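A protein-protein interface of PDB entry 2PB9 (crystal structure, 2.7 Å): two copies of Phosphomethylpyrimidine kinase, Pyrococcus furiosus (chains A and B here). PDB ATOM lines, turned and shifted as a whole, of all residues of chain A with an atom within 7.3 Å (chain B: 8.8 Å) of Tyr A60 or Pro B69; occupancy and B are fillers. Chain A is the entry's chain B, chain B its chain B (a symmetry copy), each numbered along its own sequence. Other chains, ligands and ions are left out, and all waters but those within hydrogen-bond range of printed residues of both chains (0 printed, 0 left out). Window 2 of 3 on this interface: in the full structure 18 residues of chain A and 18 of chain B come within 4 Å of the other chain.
NZ of Lys A65 lies within hydrogen-bond range of O of Val B67 (2.8 Å).
The side-chain hydroxyl (OH) of Tyr A60 is in hydrogen-bond range of the side-chain amino group (NZ) of Lys A65 (3.2 Å).
The backbone carbonyl oxygen (O) of Pro B69 sits at hydrogen-bond distance from the backbone NH (N) of Lys B54, 3.1 Å away.
The backbone carbonyl oxygen (O) of Val A58 lies within hydrogen-bond range of the backbone NH (N) of Lys A65 (2.7 Å).
The backbone NH of Gly B68 lies within hydrogen-bond range of the backbone carbonyl oxygen of Lys B54 (2.6 Å).
O of Arg B56 lies within hydrogen-bond range of N of Val B67 (2.8 Å).
Among the printed residues, merely in contact across the chains: Lys A59 with Gly B55 (3.9 Å), Tyr A60 with Lys B54 (3.3 Å), Tyr A60 with Val B67 (3.7 Å), Tyr A60 with Gly B68 (3.5 Å), Tyr A60 with Pro B69 (3.5 Å) and Gly A61 with Lys B54 (3.8 Å).
Tyr A60 touches just these residues of chain B: Lys B54, Val B67, Gly B68 and Pro B69.
Of the printed residues of chain A, Pro B69 touches Tyr A60.
Of chain B, only Lys B54 (3.8 Å) comes within 4 Å of Gly A61.
Of the printed residues of chain B, Lys A65 touches Val B67.
Of the printed residues of chain A, Gly B68 touches Tyr A60.
Of the printed residues of chain A, Gly B55 touches Lys A59 (3.9 Å).
Printed residues of chain A within 4 Å of Val B67: Tyr A60 (3.7 Å) and Lys A65 (2.8 Å).
Val B70 touches none of the printed residues of chain A.
Phe B72 touches none of the printed residues of chain A.
The nearest residue of chain B that does not touch Tyr A60 is Gly B55 (4.4 Å).
The nearest residue of chain A that does not touch Pro B69 is Lys A65 (6.0 Å).
Printed residues of chain A that touch a printed residue of chain B: Lys A59, Tyr A60, Gly A61 and Lys A65.
Of the 22 printed residues of chain B, 5 touch a printed residue of chain A.
Among the printed residues, 7 pairs touch across the chains.
Among the printed residues, no Asp or Glu carboxylate lies within 4 Å of a Lys or Arg side-chain nitrogen of the other chain.
No position is printed for both chains.
Of the 7 pairs that touch across the chains among the printed residues, none has its exchanged pair printed and touching as well.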
ATOM      1  N   VAL A  25      37.294 -20.719 -21.149  1.00  0.00           N
ATOM      2  CA  VAL A  25      36.346 -21.237 -20.165  1.00  0.00           C
ATOM      3  C   VAL A  25      36.507 -20.669 -18.771  1.00  0.00           C
ATOM      4  O   VAL A  25      35.533 -20.192 -18.183  1.00  0.00           O
ATOM      5  CB  VAL A  25      36.388 -22.786 -20.038  1.00  0.00           C
ATOM      6  CG1 VAL A  25      35.320 -23.389 -20.897  1.00  0.00           C
ATOM      7  CG2 VAL A  25      37.756 -23.327 -20.422  1.00  0.00           C
ATOM      8  N   ILE A  28      34.771 -17.310 -17.832  1.00  0.00           N
ATOM      9  CA  ILE A  28      33.335 -17.108 -17.978  1.00  0.00           C
ATOM     10  C   ILE A  28      32.648 -17.223 -16.604  1.00  0.00           C
ATOM     11  O   ILE A  28      32.955 -18.132 -15.827  1.00  0.00           O
ATOM     12  CB  ILE A  28      32.713 -18.174 -18.912  1.00  0.00           C
ATOM     13  CG1 ILE A  28      33.481 -18.245 -20.233  1.00  0.00           C
ATOM     14  CG2 ILE A  28      31.254 -17.851 -19.171  1.00  0.00           C
ATOM     15  CD1 ILE A  28      33.373 -17.001 -21.083  1.00  0.00           C
ATOM     16  N   ILE A  57      27.444 -15.338 -24.035  1.00  0.00           N
ATOM     17  CA  ILE A  57      28.357 -16.441 -24.279  1.00  0.00           C
ATOM     18  C   ILE A  57      28.446 -17.140 -22.928  1.00  0.00           C
ATOM     19  O   ILE A  57      28.719 -16.500 -21.903  1.00  0.00           O
ATOM     20  CB  ILE A  57      29.744 -15.927 -24.683  1.00  0.00           C
ATOM     21  CG1 ILE A  57      29.603 -14.977 -25.872  1.00  0.00           C
ATOM     22  CG2 ILE A  57      30.650 -17.093 -25.034  1.00  0.00           C
ATOM     23  CD1 ILE A  57      30.706 -13.932 -25.975  1.00  0.00           C
ATOM     24  N   VAL A  58      28.199 -18.443 -22.917  1.00  0.00           N
ATOM     25  CA  VAL A  58      28.232 -19.198 -21.661  1.00  0.00           C
ATOM     26  C   VAL A  58      29.167 -20.394 -21.710  1.00  0.00           C
ATOM     27  O   VAL A  58      29.681 -20.754 -22.774  1.00  0.00           O
ATOM     28  CB  VAL A  58      26.816 -19.717 -21.295  1.00  0.00           C
ATOM     29  CG1 VAL A  58      25.818 -18.565 -21.303  1.00  0.00           C
ATOM     30  CG2 VAL A  58      26.381 -20.805 -22.284  1.00  0.00           C
ATOM     31  N   LYS A  59      29.380 -21.010 -20.552  1.00  0.00           N
ATOM     32  CA  LYS A  59      30.238 -22.192 -20.472  1.00  0.00           C
ATOM     33  C   LYS A  59      29.500 -23.400 -21.048  1.00  0.00           C
ATOM     34  O   LYS A  59      28.371 -23.680 -20.652  1.00  0.00           O
ATOM     35  CB  LYS A  59      30.602 -22.508 -19.019  1.00  0.00           C
ATOM     36  CG  LYS A  59      31.378 -21.439 -18.297  1.00  0.00           C
ATOM     37  CD  LYS A  59      31.934 -21.985 -16.985  1.00  0.00           C
ATOM     38  CE  LYS A  59      30.833 -22.261 -15.957  1.00  0.00           C
ATOM     39  NZ  LYS A  59      30.160 -21.012 -15.500  1.00  0.00           N
ATOM     40  N   TYR A  60      30.121 -24.104 -21.987  1.00  0.00           N
ATOM     41  CA  TYR A  60      29.500 -25.293 -22.555  1.00  0.00           C
ATOM     42  C   TYR A  60      30.117 -26.457 -21.771  1.00  0.00           C
ATOM     43  O   TYR A  60      29.769 -26.689 -20.608  1.00  0.00           O
ATOM     44  CB  TYR A  60      29.819 -25.413 -24.047  1.00  0.00           C
ATOM     45  CG  TYR A  60      28.689 -25.989 -24.900  1.00  0.00           C
ATOM     46  CD1 TYR A  60      28.978 -26.797 -26.006  1.00  0.00           C
ATOM     47  CD2 TYR A  60      27.339 -25.730 -24.610  1.00  0.00           C
ATOM     48  CE1 TYR A  60      27.967 -27.339 -26.797  1.00  0.00           C
ATOM     49  CE2 TYR A  60      26.310 -26.274 -25.409  1.00  0.00           C
ATOM     50  CZ  TYR A  60      26.644 -27.081 -26.501  1.00  0.00           C
ATOM     51  OH  TYR A  60      25.680 -27.652 -27.307  1.00  0.00           O
ATOM     52  N   GLY A  61      31.040 -27.180 -22.386  1.00  0.00           N
ATOM     53  CA  GLY A  61      31.675 -28.271 -21.672  1.00  0.00           C
ATOM     54  C   GLY A  61      32.964 -27.666 -21.179  1.00  0.00           C
ATOM     55  O   GLY A  61      32.955 -26.796 -20.313  1.00  0.00           O
ATOM     56  N   ASN A  62      34.077 -28.123 -21.733  1.00  0.00           N
ATOM     57  CA  ASN A  62      35.378 -27.571 -21.388  1.00  0.00           C
ATOM     58  C   ASN A  62      35.612 -26.553 -22.489  1.00  0.00           C
ATOM     59  O   ASN A  62      36.661 -26.527 -23.128  1.00  0.00           O
ATOM     60  CB  ASN A  62      36.458 -28.660 -21.420  1.00  0.00           C
ATOM     61  CG  ASN A  62      36.580 -29.399 -20.097  1.00  0.00           C
ATOM     62  OD1 ASN A  62      35.606 -29.520 -19.342  1.00  0.00           O
ATOM     63  ND2 ASN A  62      37.779 -29.909 -19.810  1.00  0.00           N
ATOM     64  N   SER A  63      34.594 -25.738 -22.727  1.00  0.00           N
ATOM     65  CA  SER A  63      34.653 -24.711 -23.751  1.00  0.00           C
ATOM     66  C   SER A  63      33.519 -23.723 -23.520  1.00  0.00           C
ATOM     67  O   SER A  63      32.663 -23.940 -22.668  1.00  0.00           O
ATOM     68  CB  SER A  63      34.528 -25.343 -25.134  1.00  0.00           C
ATOM     69  OG  SER A  63      33.467 -24.747 -25.853  1.00  0.00           O
ATOM     70  N   VAL A  64      33.513 -22.637 -24.279  1.00  0.00           N
ATOM     71  CA  VAL A  64      32.486 -21.618 -24.135  1.00  0.00           C
ATOM     72  C   VAL A  64      31.608 -21.616 -25.383  1.00  0.00           C
ATOM     73  O   VAL A  64      31.977 -22.195 -26.401  1.00  0.00           O
ATOM     74  CB  VAL A  64      33.131 -20.222 -23.956  1.00  0.00           C
ATOM     75  CG1 VAL A  64      34.341 -20.326 -23.043  1.00  0.00           C
ATOM     76  CG2 VAL A  64      33.531 -19.648 -25.305  1.00  0.00           C
ATOM     77  N   LYS A  65      30.451 -20.966 -25.309  1.00  0.00           N
ATOM     78  CA  LYS A  65      29.564 -20.915 -26.459  1.00  0.00           C
ATOM     79  C   LYS A  65      28.639 -19.701 -26.498  1.00  0.00           C
ATOM     80  O   LYS A  65      28.004 -19.343 -25.506  1.00  0.00           O
ATOM     81  CB  LYS A  65      28.731 -22.196 -26.526  1.00  0.00           C
ATOM     82  CG  LYS A  65      27.624 -22.184 -27.580  1.00  0.00           C
ATOM     83  CD  LYS A  65      26.871 -23.519 -27.592  1.00  0.00           C
ATOM     84  CE  LYS A  65      25.723 -23.531 -28.603  1.00  0.00           C
ATOM     85  NZ  LYS A  65      24.976 -24.832 -28.618  1.00  0.00           N
ATOM     86  N   TYR B   9      16.625 -39.988 -20.994  1.00  0.00           N
ATOM     87  CA  TYR B   9      16.992 -39.012 -21.999  1.00  0.00           C
ATOM     88  C   TYR B   9      15.738 -38.502 -22.701  1.00  0.00           C
ATOM     89  O   TYR B   9      15.494 -37.294 -22.759  1.00  0.00           O
ATOM     90  CB  TYR B   9      17.949 -39.645 -23.016  1.00  0.00           C
ATOM     91  CG  TYR B   9      18.164 -38.804 -24.250  1.00  0.00           C
ATOM     92  CD1 TYR B   9      18.958 -37.654 -24.212  1.00  0.00           C
ATOM     93  CD2 TYR B   9      17.496 -39.108 -25.435  1.00  0.00           C
ATOM     94  CE1 TYR B   9      19.068 -36.825 -25.326  1.00  0.00           C
ATOM     95  CE2 TYR B   9      17.598 -38.291 -26.544  1.00  0.00           C
ATOM     96  CZ  TYR B   9      18.379 -37.153 -26.490  1.00  0.00           C
ATOM     97  OH  TYR B   9      18.457 -36.355 -27.606  1.00  0.00           O
ATOM     98  N   LEU B  12      13.336 -36.296 -20.249  1.00  0.00           N
ATOM     99  CA  LEU B  12      13.881 -34.988 -19.908  1.00  0.00           C
ATOM    100  C   LEU B  12      13.887 -34.098 -21.145  1.00  0.00           C
ATOM    101  O   LEU B  12      13.481 -32.933 -21.088  1.00  0.00           O
ATOM    102  CB  LEU B  12      15.301 -35.124 -19.347  1.00  0.00           C
ATOM    103  CG  LEU B  12      16.048 -33.829 -18.993  1.00  0.00           C
ATOM    104  CD1 LEU B  12      15.156 -32.866 -18.227  1.00  0.00           C
ATOM    105  CD2 LEU B  12      17.257 -34.180 -18.176  1.00  0.00           C
ATOM    106  N   THR B  13      14.330 -34.664 -22.263  1.00  0.00           N
ATOM    107  CA  THR B  13      14.392 -33.929 -23.522  1.00  0.00           C
ATOM    108  C   THR B  13      13.035 -33.358 -23.934  1.00  0.00           C
ATOM    109  O   THR B  13      12.950 -32.276 -24.511  1.00  0.00           O
ATOM    110  CB  THR B  13      14.916 -34.830 -24.637  1.00  0.00           C
ATOM    111  OG1 THR B  13      16.237 -35.280 -24.301  1.00  0.00           O
ATOM    112  CG2 THR B  13      14.947 -34.082 -25.949  1.00  0.00           C
ATOM    113  N   VAL B  16      11.972 -30.553 -21.379  1.00  0.00           N
ATOM    114  CA  VAL B  16      12.764 -29.367 -21.683  1.00  0.00           C
ATOM    115  C   VAL B  16      12.163 -28.632 -22.868  1.00  0.00           C
ATOM    116  O   VAL B  16      12.017 -27.416 -22.849  1.00  0.00           O
ATOM    117  CB  VAL B  16      14.220 -29.739 -22.030  1.00  0.00           C
ATOM    118  CG1 VAL B  16      14.986 -28.487 -22.409  1.00  0.00           C
ATOM    119  CG2 VAL B  16      14.884 -30.437 -20.851  1.00  0.00           C
ATOM    120  N   ASN B  34      18.460 -25.003 -15.015  1.00  0.00           N
ATOM    121  CA  ASN B  34      18.825 -26.352 -15.405  1.00  0.00           C
ATOM    122  C   ASN B  34      17.687 -27.302 -14.983  1.00  0.00           C
ATOM    123  O   ASN B  34      16.967 -27.052 -14.012  1.00  0.00           O
ATOM    124  CB  ASN B  34      20.159 -26.768 -14.793  1.00  0.00           C
ATOM    125  CG  ASN B  34      20.903 -27.766 -15.665  1.00  0.00           C
ATOM    126  OD1 ASN B  34      22.107 -27.969 -15.507  1.00  0.00           O
ATOM    127  ND2 ASN B  34      20.194 -28.390 -16.591  1.00  0.00           N
ATOM    128  N   PHE B  35      17.526 -28.373 -15.746  1.00  0.00           N
ATOM    129  CA  PHE B  35      16.478 -29.358 -15.539  1.00  0.00           C
ATOM    130  C   PHE B  35      17.176 -30.704 -15.603  1.00  0.00           C
ATOM    131  O   PHE B  35      17.659 -31.086 -16.663  1.00  0.00           O
ATOM    132  CB  PHE B  35      15.476 -29.222 -16.687  1.00  0.00           C
ATOM    133  CG  PHE B  35      14.133 -29.830 -16.420  1.00  0.00           C
ATOM    134  CD1 PHE B  35      13.046 -29.488 -17.233  1.00  0.00           C
ATOM    135  CD2 PHE B  35      13.940 -30.726 -15.372  1.00  0.00           C
ATOM    136  CE1 PHE B  35      11.786 -30.027 -17.003  1.00  0.00           C
ATOM    137  CE2 PHE B  35      12.682 -31.276 -15.128  1.00  0.00           C
ATOM    138  CZ  PHE B  35      11.601 -30.925 -15.943  1.00  0.00           C
ATOM    139  N   ALA B  51      21.148 -36.893 -15.800  1.00  0.00           N
ATOM    140  CA  ALA B  51      21.037 -36.226 -17.089  1.00  0.00           C
ATOM    141  C   ALA B  51      20.673 -34.748 -16.929  1.00  0.00           C
ATOM    142  O   ALA B  51      19.878 -34.379 -16.064  1.00  0.00           O
ATOM    143  CB  ALA B  51      20.003 -36.932 -17.944  1.00  0.00           C
ATOM    144  N   GLY B  52      21.254 -33.902 -17.768  1.00  0.00           N
ATOM    145  CA  GLY B  52      20.960 -32.486 -17.684  1.00  0.00           C
ATOM    146  C   GLY B  52      21.156 -31.748 -18.996  1.00  0.00           C
ATOM    147  O   GLY B  52      21.674 -32.307 -19.968  1.00  0.00           O
ATOM    148  N   VAL B  53      20.735 -30.486 -19.014  1.00  0.00           N
ATOM    149  CA  VAL B  53      20.849 -29.644 -20.196  1.00  0.00           C
ATOM    150  C   VAL B  53      22.237 -29.013 -20.269  1.00  0.00           C
ATOM    151  O   VAL B  53      22.620 -28.235 -19.391  1.00  0.00           O
ATOM    152  CB  VAL B  53      19.794 -28.509 -20.171  1.00  0.00           C
ATOM    153  CG1 VAL B  53      19.870 -27.687 -21.447  1.00  0.00           C
ATOM    154  CG2 VAL B  53      18.416 -29.093 -20.009  1.00  0.00           C
ATOM    155  N   LYS B  54      22.990 -29.348 -21.314  1.00  0.00           N
ATOM    156  CA  LYS B  54      24.331 -28.791 -21.485  1.00  0.00           C
ATOM    157  C   LYS B  54      24.219 -27.290 -21.785  1.00  0.00           C
ATOM    158  O   LYS B  54      23.588 -26.887 -22.758  1.00  0.00           O
ATOM    159  CB  LYS B  54      25.051 -29.506 -22.625  1.00  0.00           C
ATOM    160  CG  LYS B  54      26.536 -29.243 -22.681  1.00  0.00           C
ATOM    161  CD  LYS B  54      27.148 -29.890 -23.905  1.00  0.00           C
ATOM    162  CE  LYS B  54      28.601 -29.496 -24.052  1.00  0.00           C
ATOM    163  NZ  LYS B  54      29.180 -30.065 -25.298  1.00  0.00           N
ATOM    164  N   GLY B  55      24.825 -26.466 -20.935  1.00  0.00           N
ATOM    165  CA  GLY B  55      24.749 -25.030 -21.132  1.00  0.00           C
ATOM    166  C   GLY B  55      23.423 -24.494 -20.622  1.00  0.00           C
ATOM    167  O   GLY B  55      23.085 -23.327 -20.834  1.00  0.00           O
ATOM    168  N   ARG B  56      22.671 -25.368 -19.952  1.00  0.00           N
ATOM    169  CA  ARG B  56      21.363 -25.045 -19.373  1.00  0.00           C
ATOM    170  C   ARG B  56      20.399 -24.368 -20.331  1.00  0.00           C
ATOM    171  O   ARG B  56      20.605 -24.336 -21.541  1.00  0.00           O
ATOM    172  CB  ARG B  56      21.523 -24.140 -18.150  1.00  0.00           C
ATOM    173  CG  ARG B  56      22.431 -24.692 -17.098  1.00  0.00           C
ATOM    174  CD  ARG B  56      22.920 -23.576 -16.209  1.00  0.00           C
ATOM    175  NE  ARG B  56      24.143 -23.966 -15.529  1.00  0.00           N
ATOM    176  CZ  ARG B  56      25.039 -23.109 -15.055  1.00  0.00           C
ATOM    177  NH1 ARG B  56      24.833 -21.808 -15.189  1.00  0.00           N
ATOM    178  NH2 ARG B  56      26.147 -23.558 -14.465  1.00  0.00           N
ATOM    179  N   ALA B  66      17.167 -23.400 -24.592  1.00  0.00           N
ATOM    180  CA  ALA B  66      18.063 -24.460 -24.159  1.00  0.00           C
ATOM    181  C   ALA B  66      19.334 -24.288 -24.986  1.00  0.00           C
ATOM    182  O   ALA B  66      19.291 -24.293 -26.212  1.00  0.00           O
ATOM    183  CB  ALA B  66      17.439 -25.818 -24.434  1.00  0.00           C
ATOM    184  N   VAL B  67      20.463 -24.137 -24.314  1.00  0.00           N
ATOM    185  CA  VAL B  67      21.731 -23.942 -24.995  1.00  0.00           C
ATOM    186  C   VAL B  67      22.346 -25.203 -25.598  1.00  0.00           C
ATOM    187  O   VAL B  67      22.962 -25.147 -26.662  1.00  0.00           O
ATOM    188  CB  VAL B  67      22.744 -23.278 -24.037  1.00  0.00           C
ATOM    189  CG1 VAL B  67      24.151 -23.292 -24.639  1.00  0.00           C
ATOM    190  CG2 VAL B  67      22.293 -21.856 -23.748  1.00  0.00           C
ATOM    191  N   GLY B  68      22.188 -26.336 -24.924  1.00  0.00           N
ATOM    192  CA  GLY B  68      22.763 -27.570 -25.432  1.00  0.00           C
ATOM    193  C   GLY B  68      21.795 -28.728 -25.329  1.00  0.00           C
ATOM    194  O   GLY B  68      20.667 -28.542 -24.875  1.00  0.00           O
ATOM    195  N   PRO B  69      22.198 -29.935 -25.759  1.00  0.00           N
ATOM    196  CA  PRO B  69      21.327 -31.111 -25.694  1.00  0.00           C
ATOM    197  C   PRO B  69      21.419 -31.773 -24.322  1.00  0.00           C
ATOM    198  O   PRO B  69      22.307 -31.451 -23.527  1.00  0.00           O
ATOM    199  CB  PRO B  69      21.884 -32.000 -26.785  1.00  0.00           C
ATOM    200  CG  PRO B  69      23.338 -31.788 -26.610  1.00  0.00           C
ATOM    201  CD  PRO B  69      23.446 -30.264 -26.467  1.00  0.00           C
ATOM    202  N   VAL B  70      20.495 -32.690 -24.055  1.00  0.00           N
ATOM    203  CA  VAL B  70      20.476 -33.409 -22.795  1.00  0.00           C
ATOM    204  C   VAL B  70      21.584 -34.458 -22.806  1.00  0.00           C
ATOM    205  O   VAL B  70      21.711 -35.237 -23.756  1.00  0.00           O
ATOM    206  CB  VAL B  70      19.110 -34.094 -22.573  1.00  0.00           C
ATOM    207  CG1 VAL B  70      19.200 -35.079 -21.421  1.00  0.00           C
ATOM    208  CG2 VAL B  70      18.040 -33.040 -22.282  1.00  0.00           C
ATOM    209  N   GLU B  71      22.398 -34.464 -21.758  1.00  0.00           N
ATOM    210  CA  GLU B  71      23.495 -35.418 -21.649  1.00  0.00           C
ATOM    211  C   GLU B  71      23.728 -35.756 -20.180  1.00  0.00           C
ATOM    212  O   GLU B  71      23.431 -34.961 -19.292  1.00  0.00           O
ATOM    213  CB  GLU B  71      24.785 -34.833 -22.224  1.00  0.00           C
ATOM    214  CG  GLU B  71      24.629 -34.026 -23.498  1.00  0.00           C
ATOM    215  CD  GLU B  71      25.970 -33.730 -24.159  1.00  0.00           C
ATOM    216  OE1 GLU B  71      26.936 -33.394 -23.433  1.00  0.00           O
ATOM    217  OE2 GLU B  71      26.051 -33.825 -25.405  1.00  0.00           O
ATOM    218  N   PHE B  72      24.270 -36.942 -19.933  1.00  0.00           N
ATOM    219  CA  PHE B  72      24.547 -37.386 -18.578  1.00  0.00           C
ATOM    220  C   PHE B  72      25.776 -36.684 -18.069  1.00  0.00           C
ATOM    221  O   PHE B  72      26.841 -36.737 -18.687  1.00  0.00           O
ATOM    222  CB  PHE B  72      24.748 -38.906 -18.543  1.00  0.00           C
ATOM    223  CG  PHE B  72      23.475 -39.673 -18.703  1.00  0.00           C
ATOM    224  CD1 PHE B  72      22.714 -40.017 -17.589  1.00  0.00           C
ATOM    225  CD2 PHE B  72      22.978 -39.958 -19.971  1.00  0.00           C
ATOM    226  CE1 PHE B  72      21.475 -40.624 -17.732  1.00  0.00           C
ATOM    227  CE2 PHE B  72      21.736 -40.567 -20.126  1.00  0.00           C
ATOM    228  CZ  PHE B  72      20.981 -40.899 -19.003  1.00  0.00           C
ATOM    229  N   GLY B  73      25.615 -36.011 -16.937  1.00  0.00           N
ATOM    230  CA  GLY B  73      26.721 -35.286 -16.343  1.00  0.00           C
ATOM    231  C   GLY B  73      26.694 -33.813 -16.699  1.00  0.00           C
ATOM    232  O   GLY B  73      27.485 -33.043 -16.164  1.00  0.00           O
ATOM    233  N   ALA B  74      25.797 -33.423 -17.601  1.00  0.00           N
ATOM    234  CA  ALA B  74      25.683 -32.030 -18.016  1.00  0.00           C
ATOM    235  C   ALA B  74      25.611 -31.097 -16.804  1.00  0.00           C
ATOM    236  O   ALA B  74      26.286 -30.074 -16.760  1.00  0.00           O
ATOM    237  CB  ALA B  74      24.447 -31.844 -18.899  1.00  0.00           C
ATOM    238  N   SER B  75      24.794 -31.460 -15.823  1.00  0.00           N
ATOM    239  CA  SER B  75      24.656 -30.661 -14.618  1.00  0.00           C
ATOM    240  C   SER B  75      25.650 -31.068 -13.549  1.00  0.00           C
ATOM    241  O   SER B  75      26.254 -32.136 -13.609  1.00  0.00           O
ATOM    242  CB  SER B  75      23.258 -30.787 -14.031  1.00  0.00           C
ATOM    243  OG  SER B  75      23.216 -30.126 -12.778  1.00  0.00           O
